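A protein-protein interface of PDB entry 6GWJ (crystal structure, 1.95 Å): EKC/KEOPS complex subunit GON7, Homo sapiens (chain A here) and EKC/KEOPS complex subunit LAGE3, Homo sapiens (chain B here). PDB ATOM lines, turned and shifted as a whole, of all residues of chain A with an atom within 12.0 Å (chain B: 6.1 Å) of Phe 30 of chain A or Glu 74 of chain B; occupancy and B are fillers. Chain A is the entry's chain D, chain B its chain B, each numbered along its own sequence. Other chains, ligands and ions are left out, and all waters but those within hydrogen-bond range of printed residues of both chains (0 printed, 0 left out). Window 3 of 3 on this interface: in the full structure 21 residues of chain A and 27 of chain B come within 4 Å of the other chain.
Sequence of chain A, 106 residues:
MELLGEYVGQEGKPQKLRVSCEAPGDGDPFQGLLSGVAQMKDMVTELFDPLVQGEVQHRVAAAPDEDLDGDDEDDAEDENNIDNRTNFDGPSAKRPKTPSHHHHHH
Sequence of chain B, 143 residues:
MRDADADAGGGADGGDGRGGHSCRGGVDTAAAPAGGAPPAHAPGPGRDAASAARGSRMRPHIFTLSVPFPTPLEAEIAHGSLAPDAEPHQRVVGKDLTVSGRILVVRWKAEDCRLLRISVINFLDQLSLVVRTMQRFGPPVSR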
ATOM      1  N   MET A   1      -6.384  -6.974   6.493  1.00  0.00           N
ATOM      2  CA  MET A   1      -5.706  -8.269   6.555  1.00  0.00           C
ATOM      3  C   MET A   1      -4.623  -8.308   7.649  1.00  0.00           C
ATOM      4  O   MET A   1      -4.819  -8.974   8.670  1.00  0.00           O
ATOM      5  CB  MET A   1      -5.171  -8.718   5.167  1.00  0.00           C
ATOM      6  CG  MET A   1      -4.262  -7.702   4.467  1.00  0.00           C
ATOM      7  SD  MET A   1      -4.399  -7.708   2.663  1.00  0.00           S
ATOM      8  CE  MET A   1      -5.866  -6.697   2.450  1.00  0.00           C
ATOM      9  N   LEU A   3      -1.387  -5.558   9.444  1.00  0.00           N
ATOM     10  CA  LEU A   3      -0.592  -4.337   9.544  1.00  0.00           C
ATOM     11  C   LEU A   3       0.811  -4.791   9.914  1.00  0.00           C
ATOM     12  O   LEU A   3       0.986  -5.453  10.946  1.00  0.00           O
ATOM     13  CB  LEU A   3      -1.114  -3.396  10.649  1.00  0.00           C
ATOM     14  CG  LEU A   3      -2.326  -2.556  10.342  1.00  0.00           C
ATOM     15  CD1 LEU A   3      -3.604  -3.274  10.766  1.00  0.00           C
ATOM     16  CD2 LEU A   3      -2.229  -1.221  11.035  1.00  0.00           C
ATOM     17  N   VAL A  19       0.595  -7.047  13.341  1.00  0.00           N
ATOM     18  CA  VAL A  19      -0.672  -7.010  14.076  1.00  0.00           C
ATOM     19  C   VAL A  19      -1.658  -7.907  13.334  1.00  0.00           C
ATOM     20  O   VAL A  19      -1.889  -7.712  12.137  1.00  0.00           O
ATOM     21  CB  VAL A  19      -1.271  -5.584  14.283  1.00  0.00           C
ATOM     22  CG1 VAL A  19      -2.440  -5.628  15.260  1.00  0.00           C
ATOM     23  CG2 VAL A  19      -0.230  -4.586  14.759  1.00  0.00           C
ATOM     24  N   SER A  20      -2.249  -8.873  14.063  1.00  0.00           N
ATOM     25  CA  SER A  20      -3.240  -9.829  13.562  1.00  0.00           C
ATOM     26  C   SER A  20      -4.559  -9.134  13.215  1.00  0.00           C
ATOM     27  O   SER A  20      -4.756  -8.709  12.078  1.00  0.00           O
ATOM     28  CB  SER A  20      -3.485 -10.920  14.600  1.00  0.00           C
ATOM     29  OG  SER A  20      -3.884 -10.367  15.845  1.00  0.00           O
ATOM     30  N   ALA A  23      -9.890  -9.898  11.742  1.00  0.00           N
ATOM     31  CA  ALA A  23     -10.702 -10.874  11.021  1.00  0.00           C
ATOM     32  C   ALA A  23     -11.892 -10.206  10.295  1.00  0.00           C
ATOM     33  O   ALA A  23     -12.729  -9.575  10.955  1.00  0.00           O
ATOM     34  CB  ALA A  23     -11.196 -11.955  11.974  1.00  0.00           C
ATOM     35  N   PRO A  24     -11.994 -10.325   8.941  1.00  0.00           N
ATOM     36  CA  PRO A  24     -13.126  -9.692   8.234  1.00  0.00           C
ATOM     37  C   PRO A  24     -14.430 -10.492   8.364  1.00  0.00           C
ATOM     38  O   PRO A  24     -14.848 -11.207   7.442  1.00  0.00           O
ATOM     39  CB  PRO A  24     -12.618  -9.554   6.792  1.00  0.00           C
ATOM     40  CG  PRO A  24     -11.614 -10.655   6.635  1.00  0.00           C
ATOM     41  CD  PRO A  24     -11.096 -11.037   8.002  1.00  0.00           C
ATOM     42  N   GLY A  25     -15.044 -10.369   9.540  1.00  0.00           N
ATOM     43  CA  GLY A  25     -16.289 -11.040   9.886  1.00  0.00           C
ATOM     44  C   GLY A  25     -17.457 -10.082   9.915  1.00  0.00           C
ATOM     45  O   GLY A  25     -17.573  -9.218   9.039  1.00  0.00           O
ATOM     46  N   ASP A  26     -18.331 -10.233  10.925  1.00  0.00           N
ATOM     47  CA  ASP A  26     -19.504  -9.380  11.092  1.00  0.00           C
ATOM     48  C   ASP A  26     -19.194  -7.977  11.667  1.00  0.00           C
ATOM     49  O   ASP A  26     -20.001  -7.072  11.475  1.00  0.00           O
ATOM     50  CB  ASP A  26     -20.588 -10.089  11.928  1.00  0.00           C
ATOM     51  CG  ASP A  26     -21.527 -11.014  11.169  1.00  0.00           C
ATOM     52  OD1 ASP A  26     -21.633 -10.873   9.926  1.00  0.00           O
ATOM     53  OD2 ASP A  26     -22.198 -11.843  11.824  1.00  0.00           O
ATOM     54  N   GLY A  27     -18.046  -7.817  12.343  1.00  0.00           N
ATOM     55  CA  GLY A  27     -17.626  -6.567  12.983  1.00  0.00           C
ATOM     56  C   GLY A  27     -17.300  -5.402  12.061  1.00  0.00           C
ATOM     57  O   GLY A  27     -17.119  -5.591  10.851  1.00  0.00           O
ATOM     58  N   ASP A  28     -17.224  -4.177  12.632  1.00  0.00           N
ATOM     59  CA  ASP A  28     -16.922  -2.964  11.867  1.00  0.00           C
ATOM     60  C   ASP A  28     -15.459  -2.966  11.360  1.00  0.00           C
ATOM     61  O   ASP A  28     -14.531  -3.062  12.166  1.00  0.00           O
ATOM     62  CB  ASP A  28     -17.195  -1.693  12.677  1.00  0.00           C
ATOM     63  CG  ASP A  28     -17.043  -0.435  11.844  1.00  0.00           C
ATOM     64  OD1 ASP A  28     -17.993  -0.091  11.107  1.00  0.00           O
ATOM     65  OD2 ASP A  28     -15.980   0.208  11.933  1.00  0.00           O
ATOM     66  N   PRO A  29     -15.240  -2.866  10.030  1.00  0.00           N
ATOM     67  CA  PRO A  29     -13.859  -2.916   9.510  1.00  0.00           C
ATOM     68  C   PRO A  29     -12.943  -1.804  10.048  1.00  0.00           C
ATOM     69  O   PRO A  29     -11.817  -2.107  10.448  1.00  0.00           O
ATOM     70  CB  PRO A  29     -14.048  -2.868   7.986  1.00  0.00           C
ATOM     71  CG  PRO A  29     -15.464  -3.317   7.757  1.00  0.00           C
ATOM     72  CD  PRO A  29     -16.224  -2.778   8.930  1.00  0.00           C
ATOM     73  N   PHE A  30     -13.447  -0.555  10.162  1.00  0.00           N
ATOM     74  CA  PHE A  30     -12.632   0.548  10.706  1.00  0.00           C
ATOM     75  C   PHE A  30     -12.308   0.404  12.185  1.00  0.00           C
ATOM     76  O   PHE A  30     -11.219   0.824  12.585  1.00  0.00           O
ATOM     77  CB  PHE A  30     -13.228   1.935  10.415  1.00  0.00           C
ATOM     78  CG  PHE A  30     -13.080   2.316   8.959  1.00  0.00           C
ATOM     79  CD1 PHE A  30     -11.849   2.209   8.314  1.00  0.00           C
ATOM     80  CD2 PHE A  30     -14.163   2.793   8.235  1.00  0.00           C
ATOM     81  CE1 PHE A  30     -11.716   2.551   6.967  1.00  0.00           C
ATOM     82  CE2 PHE A  30     -14.021   3.155   6.891  1.00  0.00           C
ATOM     83  CZ  PHE A  30     -12.796   3.035   6.270  1.00  0.00           C
ATOM     84  N   GLN A  31     -13.231  -0.162  12.989  1.00  0.00           N
ATOM     85  CA  GLN A  31     -12.987  -0.417  14.411  1.00  0.00           C
ATOM     86  C   GLN A  31     -11.746  -1.352  14.550  1.00  0.00           C
ATOM     87  O   GLN A  31     -10.843  -1.061  15.342  1.00  0.00           O
ATOM     88  CB  GLN A  31     -14.207  -1.056  15.090  1.00  0.00           C
ATOM     89  CG  GLN A  31     -13.999  -1.282  16.604  1.00  0.00           C
ATOM     90  CD  GLN A  31     -15.198  -1.848  17.318  1.00  0.00           C
ATOM     91  OE1 GLN A  31     -16.349  -1.683  16.900  1.00  0.00           O
ATOM     92  NE2 GLN A  31     -14.961  -2.485  18.456  1.00  0.00           N
ATOM     93  N   GLY A  32     -11.733  -2.431  13.765  1.00  0.00           N
ATOM     94  CA  GLY A  32     -10.635  -3.391  13.702  1.00  0.00           C
ATOM     95  C   GLY A  32      -9.332  -2.722  13.289  1.00  0.00           C
ATOM     96  O   GLY A  32      -8.296  -2.950  13.924  1.00  0.00           O
ATOM     97  N   LEU A  33      -9.382  -1.863  12.239  1.00  0.00           N
ATOM     98  CA  LEU A  33      -8.200  -1.120  11.761  1.00  0.00           C
ATOM     99  C   LEU A  33      -7.647  -0.171  12.845  1.00  0.00           C
ATOM    100  O   LEU A  33      -6.437  -0.148  13.053  1.00  0.00           O
ATOM    101  CB  LEU A  33      -8.479  -0.375  10.437  1.00  0.00           C
ATOM    102  CG  LEU A  33      -7.297   0.385   9.758  1.00  0.00           C
ATOM    103  CD1 LEU A  33      -6.049  -0.499   9.597  1.00  0.00           C
ATOM    104  CD2 LEU A  33      -7.717   0.945   8.409  1.00  0.00           C
ATOM    105  N   LEU A  34      -8.530   0.535  13.578  1.00  0.00           N
ATOM    106  CA  LEU A  34      -8.130   1.427  14.683  1.00  0.00           C
ATOM    107  C   LEU A  34      -7.409   0.667  15.788  1.00  0.00           C
ATOM    108  O   LEU A  34      -6.407   1.155  16.313  1.00  0.00           O
ATOM    109  CB  LEU A  34      -9.338   2.170  15.262  1.00  0.00           C
ATOM    110  CG  LEU A  34      -9.878   3.309  14.380  1.00  0.00           C
ATOM    111  CD1 LEU A  34     -11.282   3.703  14.785  1.00  0.00           C
ATOM    112  CD2 LEU A  34      -8.925   4.506  14.365  1.00  0.00           C
ATOM    113  N   SER A  35      -7.888  -0.552  16.097  1.00  0.00           N
ATOM    114  CA  SER A  35      -7.297  -1.421  17.107  1.00  0.00           C
ATOM    115  C   SER A  35      -5.878  -1.820  16.697  1.00  0.00           C
ATOM    116  O   SER A  35      -4.970  -1.736  17.523  1.00  0.00           O
ATOM    117  CB  SER A  35      -8.166  -2.650  17.346  1.00  0.00           C
ATOM    118  OG  SER A  35      -7.618  -3.425  18.398  1.00  0.00           O
ATOM    119  N   GLY A  36      -5.705  -2.170  15.418  1.00  0.00           N
ATOM    120  CA  GLY A  36      -4.422  -2.558  14.836  1.00  0.00           C
ATOM    121  C   GLY A  36      -3.378  -1.451  14.889  1.00  0.00           C
ATOM    122  O   GLY A  36      -2.216  -1.702  15.227  1.00  0.00           O
ATOM    123  N   VAL A  37      -3.799  -0.214  14.572  1.00  0.00           N
ATOM    124  CA  VAL A  37      -2.953   0.993  14.579  1.00  0.00           C
ATOM    125  C   VAL A  37      -2.471   1.285  16.010  1.00  0.00           C
ATOM    126  O   VAL A  37      -1.277   1.517  16.205  1.00  0.00           O
ATOM    127  CB  VAL A  37      -3.686   2.199  13.928  1.00  0.00           C
ATOM    128  CG1 VAL A  37      -2.905   3.504  14.097  1.00  0.00           C
ATOM    129  CG2 VAL A  37      -3.971   1.926  12.458  1.00  0.00           C
ATOM    130  N   ALA A  38      -3.389   1.217  16.998  1.00  0.00           N
ATOM    131  CA  ALA A  38      -3.083   1.413  18.416  1.00  0.00           C
ATOM    132  C   ALA A  38      -2.078   0.337  18.888  1.00  0.00           C
ATOM    133  O   ALA A  38      -1.134   0.662  19.617  1.00  0.00           O
ATOM    134  CB  ALA A  38      -4.362   1.345  19.247  1.00  0.00           C
ATOM    135  N   GLN A  39      -2.246  -0.922  18.414  1.00  0.00           N
ATOM    136  CA  GLN A  39      -1.344  -2.027  18.749  1.00  0.00           C
ATOM    137  C   GLN A  39       0.021  -1.806  18.092  1.00  0.00           C
ATOM    138  O   GLN A  39       1.040  -2.078  18.725  1.00  0.00           O
ATOM    139  CB  GLN A  39      -1.920  -3.387  18.328  1.00  0.00           C
ATOM    140  CG  GLN A  39      -3.043  -3.900  19.222  1.00  0.00           C
ATOM    141  CD  GLN A  39      -3.684  -5.155  18.668  1.00  0.00           C
ATOM    142  OE1 GLN A  39      -4.831  -5.142  18.195  1.00  0.00           O
ATOM    143  NE2 GLN A  39      -2.961  -6.268  18.712  1.00  0.00           N
ATOM    144  N   PHE B  69      -6.724  -1.338   3.960  1.00  0.00           N
ATOM    145  CA  PHE B  69      -7.983  -0.571   4.024  1.00  0.00           C
ATOM    146  C   PHE B  69      -9.132  -1.428   3.484  1.00  0.00           C
ATOM    147  O   PHE B  69      -8.853  -2.345   2.714  1.00  0.00           O
ATOM    148  CB  PHE B  69      -7.865   0.783   3.272  1.00  0.00           C
ATOM    149  CG  PHE B  69      -7.071   1.803   4.058  1.00  0.00           C
ATOM    150  CD1 PHE B  69      -5.683   1.824   3.996  1.00  0.00           C
ATOM    151  CD2 PHE B  69      -7.708   2.694   4.916  1.00  0.00           C
ATOM    152  CE1 PHE B  69      -4.947   2.724   4.767  1.00  0.00           C
ATOM    153  CE2 PHE B  69      -6.971   3.591   5.691  1.00  0.00           C
ATOM    154  CZ  PHE B  69      -5.595   3.588   5.621  1.00  0.00           C
ATOM    155  N   PRO B  70     -10.412  -1.178   3.862  1.00  0.00           N
ATOM    156  CA  PRO B  70     -11.511  -2.051   3.373  1.00  0.00           C
ATOM    157  C   PRO B  70     -11.704  -2.088   1.856  1.00  0.00           C
ATOM    158  O   PRO B  70     -12.115  -3.119   1.326  1.00  0.00           O
ATOM    159  CB  PRO B  70     -12.758  -1.504   4.079  1.00  0.00           C
ATOM    160  CG  PRO B  70     -12.236  -0.706   5.232  1.00  0.00           C
ATOM    161  CD  PRO B  70     -10.919  -0.150   4.794  1.00  0.00           C
ATOM    162  N   THR B  71     -11.441  -0.963   1.163  1.00  0.00           N
ATOM    163  CA  THR B  71     -11.605  -0.868  -0.295  1.00  0.00           C
ATOM    164  C   THR B  71     -10.414  -0.112  -0.913  1.00  0.00           C
ATOM    165  O   THR B  71      -9.860   0.760  -0.230  1.00  0.00           O
ATOM    166  CB  THR B  71     -12.892  -0.076  -0.657  1.00  0.00           C
ATOM    167  OG1 THR B  71     -12.774   1.235  -0.121  1.00  0.00           O
ATOM    168  CG2 THR B  71     -14.185  -0.745  -0.181  1.00  0.00           C
ATOM    169  N   PRO B  72     -10.069  -0.336  -2.217  1.00  0.00           N
ATOM    170  CA  PRO B  72      -8.991   0.464  -2.832  1.00  0.00           C
ATOM    171  C   PRO B  72      -9.264   1.971  -2.798  1.00  0.00           C
ATOM    172  O   PRO B  72      -8.318   2.721  -2.608  1.00  0.00           O
ATOM    173  CB  PRO B  72      -8.896  -0.086  -4.260  1.00  0.00           C
ATOM    174  CG  PRO B  72      -9.503  -1.447  -4.180  1.00  0.00           C
ATOM    175  CD  PRO B  72     -10.612  -1.314  -3.183  1.00  0.00           C
ATOM    176  N   LEU B  73     -10.538   2.408  -2.906  1.00  0.00           N
ATOM    177  CA  LEU B  73     -10.881   3.836  -2.825  1.00  0.00           C
ATOM    178  C   LEU B  73     -10.539   4.441  -1.441  1.00  0.00           C
ATOM    179  O   LEU B  73     -10.020   5.556  -1.382  1.00  0.00           O
ATOM    180  CB  LEU B  73     -12.345   4.135  -3.236  1.00  0.00           C
ATOM    181  CG  LEU B  73     -12.858   5.600  -3.030  1.00  0.00           C
ATOM    182  CD1 LEU B  73     -12.013   6.635  -3.812  1.00  0.00           C
ATOM    183  CD2 LEU B  73     -14.313   5.726  -3.426  1.00  0.00           C
ATOM    184  N   GLU B  74     -10.790   3.698  -0.349  1.00  0.00           N
ATOM    185  CA  GLU B  74     -10.444   4.178   0.984  1.00  0.00           C
ATOM    186  C   GLU B  74      -8.925   4.219   1.211  1.00  0.00           C
ATOM    187  O   GLU B  74      -8.464   5.118   1.903  1.00  0.00           O
ATOM    188  CB  GLU B  74     -11.180   3.425   2.083  1.00  0.00           C
ATOM    189  CG  GLU B  74     -12.627   3.875   2.181  1.00  0.00           C
ATOM    190  CD  GLU B  74     -13.603   2.845   2.708  1.00  0.00           C
ATOM    191  OE1 GLU B  74     -13.350   1.631   2.533  1.00  0.00           O
ATOM    192  OE2 GLU B  74     -14.630   3.256   3.294  1.00  0.00           O
ATOM    193  N   ALA B  75      -8.152   3.288   0.588  1.00  0.00           N
ATOM    194  CA  ALA B  75      -6.688   3.314   0.646  1.00  0.00           C
ATOM    195  C   ALA B  75      -6.188   4.574  -0.106  1.00  0.00           C
ATOM    196  O   ALA B  75      -5.305   5.279   0.403  1.00  0.00           O
ATOM    197  CB  ALA B  75      -6.104   2.054   0.019  1.00  0.00           C
ATOM    198  N   GLU B  76      -6.779   4.865  -1.302  1.00  0.00           N
ATOM    199  CA  GLU B  76      -6.437   6.029  -2.133  1.00  0.00           C
ATOM    200  C   GLU B  76      -6.718   7.335  -1.383  1.00  0.00           C
ATOM    201  O   GLU B  76      -5.920   8.269  -1.465  1.00  0.00           O
ATOM    202  CB  GLU B  76      -7.239   6.033  -3.438  1.00  0.00           C
ATOM    203  CG  GLU B  76      -6.820   4.981  -4.450  1.00  0.00           C
ATOM    204  CD  GLU B  76      -7.842   4.704  -5.540  1.00  0.00           C
ATOM    205  OE1 GLU B  76      -8.499   5.665  -6.007  1.00  0.00           O
ATOM    206  OE2 GLU B  76      -7.973   3.524  -5.938  1.00  0.00           O
ATOM    207  N   ILE B  77      -7.863   7.397  -0.662  1.00  0.00           N
ATOM    208  CA  ILE B  77      -8.257   8.578   0.098  1.00  0.00           C
ATOM    209  C   ILE B  77      -7.261   8.821   1.231  1.00  0.00           C
ATOM    210  O   ILE B  77      -6.817   9.952   1.415  1.00  0.00           O
ATOM    211  CB  ILE B  77      -9.733   8.533   0.575  1.00  0.00           C
ATOM    212  CG1 ILE B  77     -10.703   8.713  -0.643  1.00  0.00           C
ATOM    213  CG2 ILE B  77      -9.989   9.596   1.670  1.00  0.00           C
ATOM    214  CD1 ILE B  77     -12.204   8.591  -0.350  1.00  0.00           C
ATOM    215  N   ALA B  78      -6.880   7.753   1.955  1.00  0.00           N
ATOM    216  CA  ALA B  78      -5.907   7.865   3.044  1.00  0.00           C
ATOM    217  C   ALA B  78      -4.565   8.363   2.487  1.00  0.00           C
ATOM    218  O   ALA B  78      -3.975   9.250   3.075  1.00  0.00           O
ATOM    219  CB  ALA B  78      -5.733   6.525   3.743  1.00  0.00           C
ATOM    220  N   HIS B  79      -4.127   7.849   1.316  1.00  0.00           N
ATOM    221  CA  HIS B  79      -2.885   8.294   0.671  1.00  0.00           C
ATOM    222  C   HIS B  79      -2.991   9.782   0.312  1.00  0.00           C
ATOM    223  O   HIS B  79      -2.081  10.550   0.633  1.00  0.00           O
ATOM    224  CB  HIS B  79      -2.590   7.466  -0.599  1.00  0.00           C
ATOM    225  CG  HIS B  79      -1.367   7.926  -1.335  1.00  0.00           C
ATOM    226  ND1 HIS B  79      -1.438   8.909  -2.306  1.00  0.00           N
ATOM    227  CD2 HIS B  79      -0.078   7.528  -1.207  1.00  0.00           C
ATOM    228  CE1 HIS B  79      -0.195   9.083  -2.735  1.00  0.00           C
ATOM    229  NE2 HIS B  79       0.658   8.265  -2.111  1.00  0.00           N
ATOM    230  N   VAL B 131      -8.618   7.434   9.717  1.00  0.00           N
ATOM    231  CA  VAL B 131      -9.493   6.278   9.835  1.00  0.00           C
ATOM    232  C   VAL B 131     -10.789   6.663  10.562  1.00  0.00           C
ATOM    233  O   VAL B 131     -11.864   6.326  10.074  1.00  0.00           O
ATOM    234  CB  VAL B 131      -8.781   5.040  10.434  1.00  0.00           C
ATOM    235  CG1 VAL B 131      -9.769   3.917  10.733  1.00  0.00           C
ATOM    236  CG2 VAL B 131      -7.679   4.550   9.491  1.00  0.00           C
ATOM    237  N   MET B 134     -13.031   8.786   8.096  1.00  0.00           N
ATOM    238  CA  MET B 134     -13.670   7.909   7.117  1.00  0.00           C
ATOM    239  C   MET B 134     -14.807   7.111   7.755  1.00  0.00           C
ATOM    240  O   MET B 134     -15.854   6.958   7.146  1.00  0.00           O
ATOM    241  CB  MET B 134     -12.646   6.974   6.467  1.00  0.00           C
ATOM    242  CG  MET B 134     -11.646   7.714   5.584  1.00  0.00           C
ATOM    243  SD  MET B 134     -10.631   6.634   4.538  1.00  0.00           S
ATOM    244  CE  MET B 134      -9.931   5.571   5.755  1.00  0.00           C
ATOM    245  N   GLN B 135     -14.619   6.644   8.991  1.00  0.00           N
ATOM    246  CA  GLN B 135     -15.649   5.876   9.688  1.00  0.00           C
ATOM    247  C   GLN B 135     -16.871   6.760  10.003  1.00  0.00           C
ATOM    248  O   GLN B 135     -17.999   6.354   9.749  1.00  0.00           O
ATOM    249  CB  GLN B 135     -15.076   5.271  10.989  1.00  0.00           C
ATOM    250  CG  GLN B 135     -16.028   4.313  11.723  1.00  0.00           C
ATOM    251  CD  GLN B 135     -15.467   3.883  13.061  1.00  0.00           C
ATOM    252  OE1 GLN B 135     -15.033   4.702  13.867  1.00  0.00           O
ATOM    253  NE2 GLN B 135     -15.476   2.593  13.333  1.00  0.00           N
ATOM    254  N   PRO B 139     -19.672   6.619   4.147  1.00  0.00           N
ATOM    255  CA  PRO B 139     -18.760   6.127   3.101  1.00  0.00           C
ATOM    256  C   PRO B 139     -18.456   7.185   2.031  1.00  0.00           C
ATOM    257  O   PRO B 139     -19.195   8.171   1.931  1.00  0.00           O
ATOM    258  CB  PRO B 139     -19.518   4.903   2.541  1.00  0.00           C
ATOM    259  CG  PRO B 139     -20.960   5.239   2.742  1.00  0.00           C
ATOM    260  CD  PRO B 139     -20.999   5.969   4.065  1.00  0.00           C
ATOM    261  N   PRO B 140     -17.408   7.003   1.188  1.00  0.00           N
ATOM    262  CA  PRO B 140     -17.175   7.983   0.104  1.00  0.00           C
ATOM    263  C   PRO B 140     -18.360   8.020  -0.873  1.00  0.00           C
ATOM    264  O   PRO B 140     -18.923   6.977  -1.191  1.00  0.00           O
ATOM    265  CB  PRO B 140     -15.905   7.471  -0.596  1.00  0.00           C
ATOM    266  CG  PRO B 140     -15.322   6.434   0.299  1.00  0.00           C
ATOM    267  CD  PRO B 140     -16.426   5.897   1.146  1.00  0.00           C
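The side-chain amide nitrogen of Gln 135 of chain B sits at hydrogen-bond distance from the side-chain carboxylate of Asp 28 of chain A (2.8 Å).
Phe 30 of chain A touches five residues of chain B. Glu 74 of chain B touches one residue of chain A. Phe 69 of chain B touches just one residue of chain A: Leu 33. No residue of chain A comes within 4 Å of Thr 71 of chain B. Pro 72 of chain B touches none of the printed residues of chain A. Leu 73 of chain B touches none of the printed residues of chain A. No residue of chain A comes within 4 Å of Ala 75 of chain B. No residue of chain A comes within 4 Å of Glu 76 of chain B. No residue of chain A comes within 4 Å of Ile 77 of chain B. No residue of chain A comes within 4 Å of Ala 78 of chain B. Val 131 of chain B touches three residues of chain A. Of chain A, only Phe 30 (3.7 Å) comes within 4 Å of Met 134 of chain B. Pro 140 of chain B touches none of the printed residues of chain A. Printed residues of chain A within 4 Å of Gln 135 of chain B: Asp 28 (2.8 Å), Phe 30 (3.7 Å), Gln 31 (3.6 Å) and Leu 34 (3.99 Å). Printed residues of chain B within 4 Å of Pro 29 of chain A: Pro 70. The nearest printed residue of chain B that does not touch Pro 29 of chain A is Gln 135 of chain B (6.0 Å).
Hydrophobic or aromatic side chains of chain A that line the printed part of chain B: Pro 29, Phe 30, Leu 33 and Leu 34. Of the 16 printed residues of chain B, 6 touch a printed residue of chain A. Printed residues of chain B that touch a printed residue of chain A: Phe 69, Pro 70, Glu 74, Val 131, Met 134 and Gln 135. Among the printed residues, 12 pairs touch across the chains. Among the printed residues, no Asp or Glu carboxylate lies within 4 Å of a Lys or Arg side-chain nitrogen of the other chain.
Pro 70 of chain B touches Phe 30 of chain A (CD to CE1, 3.6 Å). Phe 30 of chain A touches Glu 74 of chain B (CZ to OE2, 3.5 Å). CG1 of Val 131 of chain B touches CD1 of Phe 30 of chain A, 3.6 Å away. CE1 of Phe 30 of chain A touches CE of Met 134 of chain B (3.7 Å). CA of Gln 135 of chain B touches CD2 of Phe 30 of chain A (3.7 Å). Gln 31 of chain A touches Gln 135 of chain B (N to NE2, 3.6 Å). Leu 33 of chain A touches Phe 69 of chain B (CD2 to CE2, 3.9 Å). Leu 33 of chain A touches Val 131 of chain B (CD2 to CG2, 3.8 Å). Leu 34 of chain A touches Val 131 of chain B. Leu 34 of chain A touches Gln 135 of chain B.
The side-chain hydroxyl of Thr 71 of chain B is in hydrogen-bond range of the side-chain carboxylate of Glu 74 of chain B, 2.7 Å away. The side-chain carboxylate (OD2) of Asp 28 of chain A sits at hydrogen-bond distance from the backbone NH (N) of Phe 30 of chain A. The backbone NH (N) of Gln 31 of chain A lies within hydrogen-bond range of the side-chain carboxylate (OD2) of Asp 28 of chain A (3.0 Å).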
